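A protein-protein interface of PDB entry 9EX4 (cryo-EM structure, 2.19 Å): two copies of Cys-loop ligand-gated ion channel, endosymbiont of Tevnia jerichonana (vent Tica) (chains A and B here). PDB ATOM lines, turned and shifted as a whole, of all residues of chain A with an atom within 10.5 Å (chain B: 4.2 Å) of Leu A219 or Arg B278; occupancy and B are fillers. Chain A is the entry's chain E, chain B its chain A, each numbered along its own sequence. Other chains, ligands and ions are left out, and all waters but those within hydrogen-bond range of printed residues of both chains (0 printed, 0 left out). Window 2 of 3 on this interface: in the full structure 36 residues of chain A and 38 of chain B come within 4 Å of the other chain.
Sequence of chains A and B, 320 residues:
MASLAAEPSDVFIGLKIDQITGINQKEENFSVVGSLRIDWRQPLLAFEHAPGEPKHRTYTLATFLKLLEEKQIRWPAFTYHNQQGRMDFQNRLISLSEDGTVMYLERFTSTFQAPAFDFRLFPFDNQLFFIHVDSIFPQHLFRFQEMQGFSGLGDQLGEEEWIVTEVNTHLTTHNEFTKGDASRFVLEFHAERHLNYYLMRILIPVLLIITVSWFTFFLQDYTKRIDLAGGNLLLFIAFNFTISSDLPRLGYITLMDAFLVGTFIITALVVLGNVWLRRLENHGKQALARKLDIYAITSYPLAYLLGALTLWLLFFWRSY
Among the printed residues, pairs that only touch across the chains: Leu A219 with Arg B278 (3.7 Å), Phe A215 with Val B275 (3.8 Å), Leu A219 with Val B275 (3.8 Å), Gln A220 with Arg B279 (3.8 Å) and Leu A219 with Ile B226 (3.97 Å).
Hydrophobic or aromatic side chains of chain B that line the printed part of chain A: Ile B226 and Val B275. Among the printed residues, 6 pairs touch across the chains. Among the printed residues, no Asp or Glu carboxylate lies within 4 Å of a Lys or Arg side-chain nitrogen of the other chain.
The guanidinium group of Arg B279 lies within hydrogen-bond range of the backbone carbonyl oxygen of Phe A218, 2.8 Å away.
Positions printed for both chains: 222, 274 and 281.
Printed residues of chain B within 4 Å of Phe A215: Val B275. Printed residues of chain B within 4 Å of Phe A218: Arg B279 (2.8 Å). Of the printed residues of chain B, Leu A219 touches Ile B226 (3.97 Å), Val B275 (3.8 Å) and Arg B278 (3.7 Å). Printed residues of chain B within 4 Å of Gln A220: Arg B279 (3.8 Å). No residue of chain A comes within 4 Å of Tyr B222. Printed residues of chain A within 4 Å of Ile B226: Leu A219. Of chain A, only Phe A215 and Leu A219 come within 4 Å of Val B275. No residue of chain A comes within 4 Å of Leu B277. Arg B278 touches just one residue of chain A: Leu A219. No residue of chain A comes within 4 Å of Glu B281. Asn B282 touches none of the printed residues of chain A. The nearest residue of chain A that does not touch Arg B278 is Lys A224 (6.8 Å). The nearest printed residue of chain A that does not touch Arg B279 is Leu A219 (4.7 Å).
The guanidinium group (NH1) of Arg B278 lies within salt-bridge range of the side-chain carboxylate (OE1) of Glu B281 (2.8 Å). The side-chain amide nitrogen (ND2) of Asn B282 sits at hydrogen-bond distance from the backbone carbonyl oxygen (O) of Arg B278, 3.4 Å away.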
ATOM      1  N   VAL A 212       6.673   0.618  -9.935  1.00  0.00           N
ATOM      2  CA  VAL A 212       5.287   1.077  -9.991  1.00  0.00           C
ATOM      3  C   VAL A 212       4.328  -0.102  -9.877  1.00  0.00           C
ATOM      4  O   VAL A 212       3.283  -0.011  -9.216  1.00  0.00           O
ATOM      5  CB  VAL A 212       5.038   1.896 -11.270  1.00  0.00           C
ATOM      6  CG1 VAL A 212       3.563   2.257 -11.384  1.00  0.00           C
ATOM      7  CG2 VAL A 212       5.884   3.150 -11.257  1.00  0.00           C
ATOM      8  N   SER A 213       4.670  -1.231 -10.503  1.00  0.00           N
ATOM      9  CA  SER A 213       3.823  -2.413 -10.394  1.00  0.00           C
ATOM     10  C   SER A 213       3.736  -2.907  -8.954  1.00  0.00           C
ATOM     11  O   SER A 213       2.668  -3.332  -8.499  1.00  0.00           O
ATOM     12  CB  SER A 213       4.345  -3.512 -11.316  1.00  0.00           C
ATOM     13  OG  SER A 213       4.256  -3.103 -12.669  1.00  0.00           O
ATOM     14  N   TRP A 214       4.855  -2.871  -8.225  1.00  0.00           N
ATOM     15  CA  TRP A 214       4.832  -3.249  -6.815  1.00  0.00           C
ATOM     16  C   TRP A 214       4.148  -2.189  -5.951  1.00  0.00           C
ATOM     17  O   TRP A 214       3.552  -2.523  -4.921  1.00  0.00           O
ATOM     18  CB  TRP A 214       6.257  -3.509  -6.329  1.00  0.00           C
ATOM     19  CG  TRP A 214       6.346  -4.017  -4.931  1.00  0.00           C
ATOM     20  CD1 TRP A 214       6.099  -5.287  -4.503  1.00  0.00           C
ATOM     21  CD2 TRP A 214       6.738  -3.271  -3.774  1.00  0.00           C
ATOM     22  NE1 TRP A 214       6.300  -5.377  -3.148  1.00  0.00           N
ATOM     23  CE2 TRP A 214       6.693  -4.152  -2.676  1.00  0.00           C
ATOM     24  CE3 TRP A 214       7.116  -1.942  -3.557  1.00  0.00           C
ATOM     25  CZ2 TRP A 214       7.011  -3.748  -1.382  1.00  0.00           C
ATOM     26  CZ3 TRP A 214       7.431  -1.542  -2.271  1.00  0.00           C
ATOM     27  CH2 TRP A 214       7.377  -2.443  -1.200  1.00  0.00           C
ATOM     28  N   PHE A 215       4.234  -0.915  -6.344  1.00  0.00           N
ATOM     29  CA  PHE A 215       3.497   0.139  -5.650  1.00  0.00           C
ATOM     30  C   PHE A 215       1.997  -0.099  -5.736  1.00  0.00           C
ATOM     31  O   PHE A 215       1.265   0.113  -4.762  1.00  0.00           O
ATOM     32  CB  PHE A 215       3.838   1.509  -6.245  1.00  0.00           C
ATOM     33  CG  PHE A 215       5.119   2.107  -5.733  1.00  0.00           C
ATOM     34  CD1 PHE A 215       5.737   1.610  -4.597  1.00  0.00           C
ATOM     35  CD2 PHE A 215       5.697   3.188  -6.382  1.00  0.00           C
ATOM     36  CE1 PHE A 215       6.912   2.170  -4.129  1.00  0.00           C
ATOM     37  CE2 PHE A 215       6.868   3.751  -5.922  1.00  0.00           C
ATOM     38  CZ  PHE A 215       7.477   3.244  -4.793  1.00  0.00           C
ATOM     39  N   THR A 216       1.523  -0.534  -6.904  1.00  0.00           N
ATOM     40  CA  THR A 216       0.096  -0.761  -7.098  1.00  0.00           C
ATOM     41  C   THR A 216      -0.442  -1.930  -6.278  1.00  0.00           C
ATOM     42  O   THR A 216      -1.665  -2.077  -6.175  1.00  0.00           O
ATOM     43  CB  THR A 216      -0.194  -0.998  -8.580  1.00  0.00           C
ATOM     44  OG1 THR A 216       0.627  -2.066  -9.063  1.00  0.00           O
ATOM     45  CG2 THR A 216       0.095   0.260  -9.390  1.00  0.00           C
ATOM     46  N   PHE A 217       0.427  -2.757  -5.691  1.00  0.00           N
ATOM     47  CA  PHE A 217      -0.033  -3.923  -4.943  1.00  0.00           C
ATOM     48  C   PHE A 217      -0.732  -3.561  -3.637  1.00  0.00           C
ATOM     49  O   PHE A 217      -1.457  -4.400  -3.091  1.00  0.00           O
ATOM     50  CB  PHE A 217       1.136  -4.863  -4.652  1.00  0.00           C
ATOM     51  CG  PHE A 217       1.489  -5.764  -5.798  1.00  0.00           C
ATOM     52  CD1 PHE A 217       0.805  -5.685  -6.997  1.00  0.00           C
ATOM     53  CD2 PHE A 217       2.495  -6.706  -5.668  1.00  0.00           C
ATOM     54  CE1 PHE A 217       1.123  -6.517  -8.050  1.00  0.00           C
ATOM     55  CE2 PHE A 217       2.819  -7.542  -6.717  1.00  0.00           C
ATOM     56  CZ  PHE A 217       2.133  -7.448  -7.910  1.00  0.00           C
ATOM     57  N   PHE A 218      -0.544  -2.347  -3.120  1.00  0.00           N
ATOM     58  CA  PHE A 218      -1.141  -1.992  -1.838  1.00  0.00           C
ATOM     59  C   PHE A 218      -2.630  -1.675  -1.934  1.00  0.00           C
ATOM     60  O   PHE A 218      -3.276  -1.489  -0.898  1.00  0.00           O
ATOM     61  CB  PHE A 218      -0.398  -0.805  -1.223  1.00  0.00           C
ATOM     62  CG  PHE A 218       0.993  -1.138  -0.761  1.00  0.00           C
ATOM     63  CD1 PHE A 218       2.066  -1.065  -1.635  1.00  0.00           C
ATOM     64  CD2 PHE A 218       1.224  -1.534   0.545  1.00  0.00           C
ATOM     65  CE1 PHE A 218       3.345  -1.375  -1.209  1.00  0.00           C
ATOM     66  CE2 PHE A 218       2.498  -1.843   0.977  1.00  0.00           C
ATOM     67  CZ  PHE A 218       3.561  -1.765   0.098  1.00  0.00           C
ATOM     68  N   LEU A 219      -3.187  -1.611  -3.146  1.00  0.00           N
ATOM     69  CA  LEU A 219      -4.617  -1.384  -3.310  1.00  0.00           C
ATOM     70  C   LEU A 219      -5.448  -2.621  -2.996  1.00  0.00           C
ATOM     71  O   LEU A 219      -6.666  -2.502  -2.833  1.00  0.00           O
ATOM     72  CB  LEU A 219      -4.917  -0.916  -4.734  1.00  0.00           C
ATOM     73  CG  LEU A 219      -4.214   0.362  -5.192  1.00  0.00           C
ATOM     74  CD1 LEU A 219      -4.585   0.688  -6.629  1.00  0.00           C
ATOM     75  CD2 LEU A 219      -4.555   1.520  -4.270  1.00  0.00           C
ATOM     76  N   GLN A 220      -4.816  -3.794  -2.912  1.00  0.00           N
ATOM     77  CA  GLN A 220      -5.507  -5.058  -2.646  1.00  0.00           C
ATOM     78  C   GLN A 220      -6.578  -5.333  -3.702  1.00  0.00           C
ATOM     79  O   GLN A 220      -7.746  -5.577  -3.388  1.00  0.00           O
ATOM     80  CB  GLN A 220      -6.104  -5.073  -1.235  1.00  0.00           C
ATOM     81  CG  GLN A 220      -5.088  -4.836  -0.127  1.00  0.00           C
ATOM     82  CD  GLN A 220      -5.727  -4.773   1.247  1.00  0.00           C
ATOM     83  OE1 GLN A 220      -6.939  -4.927   1.389  1.00  0.00           O
ATOM     84  NE2 GLN A 220      -4.909  -4.545   2.270  1.00  0.00           N
ATOM     85  N   ASP A 221      -6.169  -5.293  -4.970  1.00  0.00           N
ATOM     86  CA  ASP A 221      -7.059  -5.546  -6.103  1.00  0.00           C
ATOM     87  C   ASP A 221      -6.404  -6.589  -7.004  1.00  0.00           C
ATOM     88  O   ASP A 221      -5.541  -6.258  -7.828  1.00  0.00           O
ATOM     89  CB  ASP A 221      -7.363  -4.259  -6.864  1.00  0.00           C
ATOM     90  CG  ASP A 221      -8.611  -4.369  -7.717  1.00  0.00           C
ATOM     91  OD1 ASP A 221      -9.291  -5.414  -7.646  1.00  0.00           O
ATOM     92  OD2 ASP A 221      -8.913  -3.409  -8.456  1.00  0.00           O
ATOM     93  N   TYR A 222      -6.825  -7.846  -6.847  1.00  0.00           N
ATOM     94  CA  TYR A 222      -6.196  -8.948  -7.570  1.00  0.00           C
ATOM     95  C   TYR A 222      -6.400  -8.820  -9.075  1.00  0.00           C
ATOM     96  O   TYR A 222      -5.476  -9.074  -9.857  1.00  0.00           O
ATOM     97  CB  TYR A 222      -6.747 -10.282  -7.064  1.00  0.00           C
ATOM     98  CG  TYR A 222      -6.687 -10.445  -5.559  1.00  0.00           C
ATOM     99  CD1 TYR A 222      -5.620  -9.938  -4.826  1.00  0.00           C
ATOM    100  CD2 TYR A 222      -7.700 -11.101  -4.872  1.00  0.00           C
ATOM    101  CE1 TYR A 222      -5.564 -10.083  -3.451  1.00  0.00           C
ATOM    102  CE2 TYR A 222      -7.652 -11.250  -3.498  1.00  0.00           C
ATOM    103  CZ  TYR A 222      -6.582 -10.740  -2.794  1.00  0.00           C
ATOM    104  OH  TYR A 222      -6.531 -10.886  -1.426  1.00  0.00           O
ATOM    105  N   THR A 223      -7.608  -8.439  -9.500  1.00  0.00           N
ATOM    106  CA  THR A 223      -7.881  -8.292 -10.928  1.00  0.00           C
ATOM    107  C   THR A 223      -7.023  -7.193 -11.546  1.00  0.00           C
ATOM    108  O   THR A 223      -6.487  -7.356 -12.651  1.00  0.00           O
ATOM    109  CB  THR A 223      -9.366  -7.999 -11.148  1.00  0.00           C
ATOM    110  OG1 THR A 223     -10.152  -9.059 -10.590  1.00  0.00           O
ATOM    111  CG2 THR A 223      -9.675  -7.871 -12.632  1.00  0.00           C
ATOM    112  N   LYS A 224      -6.888  -6.064 -10.847  1.00  0.00           N
ATOM    113  CA  LYS A 224      -6.048  -4.982 -11.345  1.00  0.00           C
ATOM    114  C   LYS A 224      -4.586  -5.411 -11.410  1.00  0.00           C
ATOM    115  O   LYS A 224      -3.870  -5.050 -12.354  1.00  0.00           O
ATOM    116  CB  LYS A 224      -6.214  -3.746 -10.462  1.00  0.00           C
ATOM    117  CG  LYS A 224      -5.678  -2.466 -11.074  1.00  0.00           C
ATOM    118  CD  LYS A 224      -6.054  -1.265 -10.226  1.00  0.00           C
ATOM    119  CE  LYS A 224      -5.630   0.036 -10.886  1.00  0.00           C
ATOM    120  NZ  LYS A 224      -5.993   1.216 -10.058  1.00  0.00           N
ATOM    121  N   ARG A 225      -4.131  -6.184 -10.420  1.00  0.00           N
ATOM    122  CA  ARG A 225      -2.777  -6.725 -10.477  1.00  0.00           C
ATOM    123  C   ARG A 225      -2.591  -7.616 -11.698  1.00  0.00           C
ATOM    124  O   ARG A 225      -1.564  -7.542 -12.385  1.00  0.00           O
ATOM    125  CB  ARG A 225      -2.464  -7.507  -9.202  1.00  0.00           C
ATOM    126  CG  ARG A 225      -2.456  -6.680  -7.931  1.00  0.00           C
ATOM    127  CD  ARG A 225      -2.255  -7.573  -6.720  1.00  0.00           C
ATOM    128  NE  ARG A 225      -2.327  -6.836  -5.464  1.00  0.00           N
ATOM    129  CZ  ARG A 225      -2.192  -7.389  -4.267  1.00  0.00           C
ATOM    130  NH1 ARG A 225      -1.975  -8.686  -4.125  1.00  0.00           N
ATOM    131  NH2 ARG A 225      -2.279  -6.621  -3.184  1.00  0.00           N
ATOM    132  N   LEU A 228      -2.402  -5.407 -14.860  1.00  0.00           N
ATOM    133  CA  LEU A 228      -1.130  -4.698 -14.943  1.00  0.00           C
ATOM    134  C   LEU A 228       0.008  -5.641 -15.319  1.00  0.00           C
ATOM    135  O   LEU A 228       0.867  -5.292 -16.138  1.00  0.00           O
ATOM    136  CB  LEU A 228      -0.836  -3.995 -13.618  1.00  0.00           C
ATOM    137  CG  LEU A 228       0.380  -3.071 -13.603  1.00  0.00           C
ATOM    138  CD1 LEU A 228       0.234  -1.977 -14.648  1.00  0.00           C
ATOM    139  CD2 LEU A 228       0.570  -2.468 -12.226  1.00  0.00           C
ATOM    140  N   ASN A 274      -1.690 -14.234  -8.331  1.00  0.00           N
ATOM    141  CA  ASN A 274      -2.870 -13.380  -8.243  1.00  0.00           C
ATOM    142  C   ASN A 274      -4.132 -14.134  -8.646  1.00  0.00           C
ATOM    143  O   ASN A 274      -5.194 -13.948  -8.038  1.00  0.00           O
ATOM    144  CB  ASN A 274      -2.680 -12.135  -9.107  1.00  0.00           C
ATOM    145  CG  ASN A 274      -1.585 -11.227  -8.585  1.00  0.00           C
ATOM    146  OD1 ASN A 274      -1.321 -11.179  -7.384  1.00  0.00           O
ATOM    147  ND2 ASN A 274      -0.936 -10.501  -9.490  1.00  0.00           N
ATOM    148  N   GLU A 281     -10.612 -16.015  -3.032  1.00  0.00           N
ATOM    149  CA  GLU A 281     -11.577 -15.013  -2.588  1.00  0.00           C
ATOM    150  C   GLU A 281     -12.980 -15.328  -3.097  1.00  0.00           C
ATOM    151  O   GLU A 281     -13.968 -15.105  -2.386  1.00  0.00           O
ATOM    152  CB  GLU A 281     -11.145 -13.621  -3.046  1.00  0.00           C
ATOM    153  CG  GLU A 281     -12.002 -12.496  -2.484  1.00  0.00           C
ATOM    154  CD  GLU A 281     -11.631 -11.139  -3.049  1.00  0.00           C
ATOM    155  OE1 GLU A 281     -11.175 -11.080  -4.209  1.00  0.00           O
ATOM    156  OE2 GLU A 281     -11.794 -10.131  -2.330  1.00  0.00           O
ATOM    157  N   GLN A 286     -12.017 -15.206   1.900  1.00  0.00           N
ATOM    158  CA  GLN A 286     -11.384 -13.893   1.930  1.00  0.00           C
ATOM    159  C   GLN A 286     -10.421 -13.758   3.103  1.00  0.00           C
ATOM    160  O   GLN A 286      -9.396 -13.078   2.985  1.00  0.00           O
ATOM    161  CB  GLN A 286     -12.451 -12.799   1.988  1.00  0.00           C
ATOM    162  CG  GLN A 286     -11.917 -11.390   1.792  1.00  0.00           C
ATOM    163  CD  GLN A 286     -13.013 -10.344   1.811  1.00  0.00           C
ATOM    164  OE1 GLN A 286     -14.122 -10.599   2.284  1.00  0.00           O
ATOM    165  NE2 GLN A 286     -12.712  -9.160   1.292  1.00  0.00           N
ATOM    166  N   ARG A 290      -6.555 -12.787   2.641  1.00  0.00           N
ATOM    167  CA  ARG A 290      -5.932 -11.682   3.361  1.00  0.00           C
ATOM    168  C   ARG A 290      -4.733 -12.160   4.172  1.00  0.00           C
ATOM    169  O   ARG A 290      -3.735 -11.440   4.296  1.00  0.00           O
ATOM    170  CB  ARG A 290      -6.964 -11.002   4.261  1.00  0.00           C
ATOM    171  CG  ARG A 290      -6.486  -9.707   4.896  1.00  0.00           C
ATOM    172  CD  ARG A 290      -7.660  -8.885   5.402  1.00  0.00           C
ATOM    173  NE  ARG A 290      -8.591  -8.558   4.330  1.00  0.00           N
ATOM    174  CZ  ARG A 290      -9.687  -7.828   4.481  1.00  0.00           C
ATOM    175  NH1 ARG A 290     -10.025  -7.325   5.658  1.00  0.00           N
ATOM    176  NH2 ARG A 290     -10.464  -7.595   3.428  1.00  0.00           N
ATOM    177  N   ASP A 293      -1.937 -12.618   1.689  1.00  0.00           N
ATOM    178  CA  ASP A 293      -1.562 -11.420   0.942  1.00  0.00           C
ATOM    179  C   ASP A 293      -0.245 -10.828   1.425  1.00  0.00           C
ATOM    180  O   ASP A 293       0.524 -10.297   0.617  1.00  0.00           O
ATOM    181  CB  ASP A 293      -2.678 -10.377   1.036  1.00  0.00           C
ATOM    182  CG  ASP A 293      -2.393  -9.147   0.200  1.00  0.00           C
ATOM    183  OD1 ASP A 293      -2.347  -9.268  -1.043  1.00  0.00           O
ATOM    184  OD2 ASP A 293      -2.217  -8.056   0.783  1.00  0.00           O
ATOM    185  N   ILE A 297       2.902 -10.188  -1.015  1.00  0.00           N
ATOM    186  CA  ILE A 297       3.539  -8.888  -1.192  1.00  0.00           C
ATOM    187  C   ILE A 297       5.028  -8.968  -0.870  1.00  0.00           C
ATOM    188  O   ILE A 297       5.863  -8.421  -1.602  1.00  0.00           O
ATOM    189  CB  ILE A 297       2.830  -7.825  -0.333  1.00  0.00           C
ATOM    190  CG1 ILE A 297       1.413  -7.574  -0.853  1.00  0.00           C
ATOM    191  CG2 ILE A 297       3.627  -6.530  -0.309  1.00  0.00           C
ATOM    192  CD1 ILE A 297       0.649  -6.535  -0.060  1.00  0.00           C
ATOM    193  N   TYR B 222      -9.294   8.565  -7.814  1.00  0.00           N
ATOM    194  CA  TYR B 222      -7.915   8.142  -7.589  1.00  0.00           C
ATOM    195  C   TYR B 222      -7.513   7.016  -8.535  1.00  0.00           C
ATOM    196  O   TYR B 222      -6.395   7.009  -9.064  1.00  0.00           O
ATOM    197  CB  TYR B 222      -7.736   7.710  -6.133  1.00  0.00           C
ATOM    198  CG  TYR B 222      -8.218   8.730  -5.123  1.00  0.00           C
ATOM    199  CD1 TYR B 222      -8.065  10.092  -5.350  1.00  0.00           C
ATOM    200  CD2 TYR B 222      -8.832   8.329  -3.943  1.00  0.00           C
ATOM    201  CE1 TYR B 222      -8.507  11.026  -4.430  1.00  0.00           C
ATOM    202  CE2 TYR B 222      -9.277   9.255  -3.018  1.00  0.00           C
ATOM    203  CZ  TYR B 222      -9.112  10.601  -3.267  1.00  0.00           C
ATOM    204  OH  TYR B 222      -9.553  11.526  -2.349  1.00  0.00           O
ATOM    205  N   ILE B 226      -4.540   6.992 -11.308  1.00  0.00           N
ATOM    206  CA  ILE B 226      -3.487   5.977 -11.356  1.00  0.00           C
ATOM    207  C   ILE B 226      -3.363   5.408 -12.764  1.00  0.00           C
ATOM    208  O   ILE B 226      -2.258   5.265 -13.300  1.00  0.00           O
ATOM    209  CB  ILE B 226      -3.762   4.868 -10.324  1.00  0.00           C
ATOM    210  CG1 ILE B 226      -3.682   5.423  -8.902  1.00  0.00           C
ATOM    211  CG2 ILE B 226      -2.789   3.710 -10.506  1.00  0.00           C
ATOM    212  CD1 ILE B 226      -4.103   4.438  -7.837  1.00  0.00           C
ATOM    213  N   ASN B 274      -1.367   8.942  -5.284  1.00  0.00           N
ATOM    214  CA  ASN B 274      -2.728   8.491  -5.557  1.00  0.00           C
ATOM    215  C   ASN B 274      -3.011   7.149  -4.891  1.00  0.00           C
ATOM    216  O   ASN B 274      -4.116   6.925  -4.379  1.00  0.00           O
ATOM    217  CB  ASN B 274      -2.963   8.412  -7.064  1.00  0.00           C
ATOM    218  CG  ASN B 274      -2.934   9.773  -7.729  1.00  0.00           C
ATOM    219  OD1 ASN B 274      -3.272  10.785  -7.114  1.00  0.00           O
ATOM    220  ND2 ASN B 274      -2.528   9.807  -8.993  1.00  0.00           N
ATOM    221  N   VAL B 275      -2.028   6.244  -4.887  1.00  0.00           N
ATOM    222  CA  VAL B 275      -2.211   4.961  -4.211  1.00  0.00           C
ATOM    223  C   VAL B 275      -2.429   5.170  -2.718  1.00  0.00           C
ATOM    224  O   VAL B 275      -3.298   4.532  -2.106  1.00  0.00           O
ATOM    225  CB  VAL B 275      -1.014   4.032  -4.487  1.00  0.00           C
ATOM    226  CG1 VAL B 275      -1.056   2.821  -3.566  1.00  0.00           C
ATOM    227  CG2 VAL B 275      -1.013   3.587  -5.940  1.00  0.00           C
ATOM    228  N   TRP B 276      -1.647   6.065  -2.106  1.00  0.00           N
ATOM    229  CA  TRP B 276      -1.826   6.330  -0.680  1.00  0.00           C
ATOM    230  C   TRP B 276      -3.204   6.917  -0.394  1.00  0.00           C
ATOM    231  O   TRP B 276      -3.854   6.547   0.594  1.00  0.00           O
ATOM    232  CB  TRP B 276      -0.728   7.260  -0.168  1.00  0.00           C
ATOM    233  CG  TRP B 276      -0.779   7.476   1.318  1.00  0.00           C
ATOM    234  CD1 TRP B 276      -0.708   6.516   2.286  1.00  0.00           C
ATOM    235  CD2 TRP B 276      -0.902   8.729   2.004  1.00  0.00           C
ATOM    236  NE1 TRP B 276      -0.787   7.092   3.531  1.00  0.00           N
ATOM    237  CE2 TRP B 276      -0.905   8.449   3.386  1.00  0.00           C
ATOM    238  CE3 TRP B 276      -1.013  10.057   1.585  1.00  0.00           C
ATOM    239  CZ2 TRP B 276      -1.014   9.449   4.349  1.00  0.00           C
ATOM    240  CZ3 TRP B 276      -1.121  11.049   2.544  1.00  0.00           C
ATOM    241  CH2 TRP B 276      -1.119  10.739   3.910  1.00  0.00           C
ATOM    242  N   LEU B 277      -3.668   7.835  -1.246  1.00  0.00           N
ATOM    243  CA  LEU B 277      -4.997   8.410  -1.052  1.00  0.00           C
ATOM    244  C   LEU B 277      -6.088   7.350  -1.172  1.00  0.00           C
ATOM    245  O   LEU B 277      -7.044   7.339  -0.387  1.00  0.00           O
ATOM    246  CB  LEU B 277      -5.236   9.543  -2.051  1.00  0.00           C
ATOM    247  CG  LEU B 277      -4.497  10.854  -1.777  1.00  0.00           C
ATOM    248  CD1 LEU B 277      -4.843  11.894  -2.830  1.00  0.00           C
ATOM    249  CD2 LEU B 277      -4.821  11.368  -0.383  1.00  0.00           C
ATOM    250  N   ARG B 278      -5.964   6.452  -2.154  1.00  0.00           N
ATOM    251  CA  ARG B 278      -6.951   5.385  -2.302  1.00  0.00           C
ATOM    252  C   ARG B 278      -6.947   4.458  -1.091  1.00  0.00           C
ATOM    253  O   ARG B 278      -8.010   4.026  -0.626  1.00  0.00           O
ATOM    254  CB  ARG B 278      -6.690   4.596  -3.585  1.00  0.00           C
ATOM    255  CG  ARG B 278      -7.652   3.437  -3.806  1.00  0.00           C
ATOM    256  CD  ARG B 278      -9.099   3.908  -3.839  1.00  0.00           C
ATOM    257  NE  ARG B 278     -10.029   2.802  -4.033  1.00  0.00           N
ATOM    258  CZ  ARG B 278     -11.349   2.930  -4.075  1.00  0.00           C
ATOM    259  NH1 ARG B 278     -11.934   4.109  -3.937  1.00  0.00           N
ATOM    260  NH2 ARG B 278     -12.100   1.849  -4.260  1.00  0.00           N
ATOM    261  N   ARG B 279      -5.759   4.135  -0.572  1.00  0.00           N
ATOM    262  CA  ARG B 279      -5.686   3.284   0.613  1.00  0.00           C
ATOM    263  C   ARG B 279      -6.321   3.968   1.818  1.00  0.00           C
ATOM    264  O   ARG B 279      -6.991   3.317   2.628  1.00  0.00           O
ATOM    265  CB  ARG B 279      -4.236   2.908   0.910  1.00  0.00           C
ATOM    266  CG  ARG B 279      -4.088   1.915   2.053  1.00  0.00           C
ATOM    267  CD  ARG B 279      -2.648   1.465   2.225  1.00  0.00           C
ATOM    268  NE  ARG B 279      -2.519   0.451   3.265  1.00  0.00           N
ATOM    269  CZ  ARG B 279      -2.629  -0.854   3.058  1.00  0.00           C
ATOM    270  NH1 ARG B 279      -2.868  -1.344   1.853  1.00  0.00           N
ATOM    271  NH2 ARG B 279      -2.495  -1.687   4.085  1.00  0.00           N
ATOM    272  N   LEU B 280      -6.113   5.280   1.958  1.00  0.00           N
ATOM    273  CA  LEU B 280      -6.775   6.016   3.032  1.00  0.00           C
ATOM    274  C   LEU B 280      -8.290   5.976   2.875  1.00  0.00           C
ATOM    275  O   LEU B 280      -9.019   5.800   3.858  1.00  0.00           O
ATOM    276  CB  LEU B 280      -6.281   7.462   3.069  1.00  0.00           C
ATOM    277  CG  LEU B 280      -4.904   7.708   3.685  1.00  0.00           C
ATOM    278  CD1 LEU B 280      -4.573   9.191   3.663  1.00  0.00           C
ATOM    279  CD2 LEU B 280      -4.851   7.164   5.104  1.00  0.00           C
ATOM    280  N   GLU B 281      -8.782   6.142   1.645  1.00  0.00           N
ATOM    281  CA  GLU B 281     -10.225   6.122   1.419  1.00  0.00           C
ATOM    282  C   GLU B 281     -10.818   4.751   1.728  1.00  0.00           C
ATOM    283  O   GLU B 281     -11.934   4.658   2.254  1.00  0.00           O
ATOM    284  CB  GLU B 281     -10.541   6.527  -0.020  1.00  0.00           C
ATOM    285  CG  GLU B 281     -12.027   6.697  -0.298  1.00  0.00           C
ATOM    286  CD  GLU B 281     -12.323   6.977  -1.758  1.00  0.00           C
ATOM    287  OE1 GLU B 281     -11.559   6.501  -2.623  1.00  0.00           O
ATOM    288  OE2 GLU B 281     -13.318   7.676  -2.041  1.00  0.00           O
ATOM    289  N   ASN B 282     -10.091   3.679   1.407  1.00  0.00           N
ATOM    290  CA  ASN B 282     -10.621   2.331   1.596  1.00  0.00           C
ATOM    291  C   ASN B 282     -10.852   1.978   3.063  1.00  0.00           C
ATOM    292  O   ASN B 282     -11.598   1.034   3.344  1.00  0.00           O
ATOM    293  CB  ASN B 282      -9.684   1.299   0.966  1.00  0.00           C
ATOM    294  CG  ASN B 282      -9.895   1.156  -0.527  1.00  0.00           C
ATOM    295  OD1 ASN B 282     -10.993   1.382  -1.035  1.00  0.00           O
ATOM    296  ND2 ASN B 282      -8.842   0.771  -1.240  1.00  0.00           N
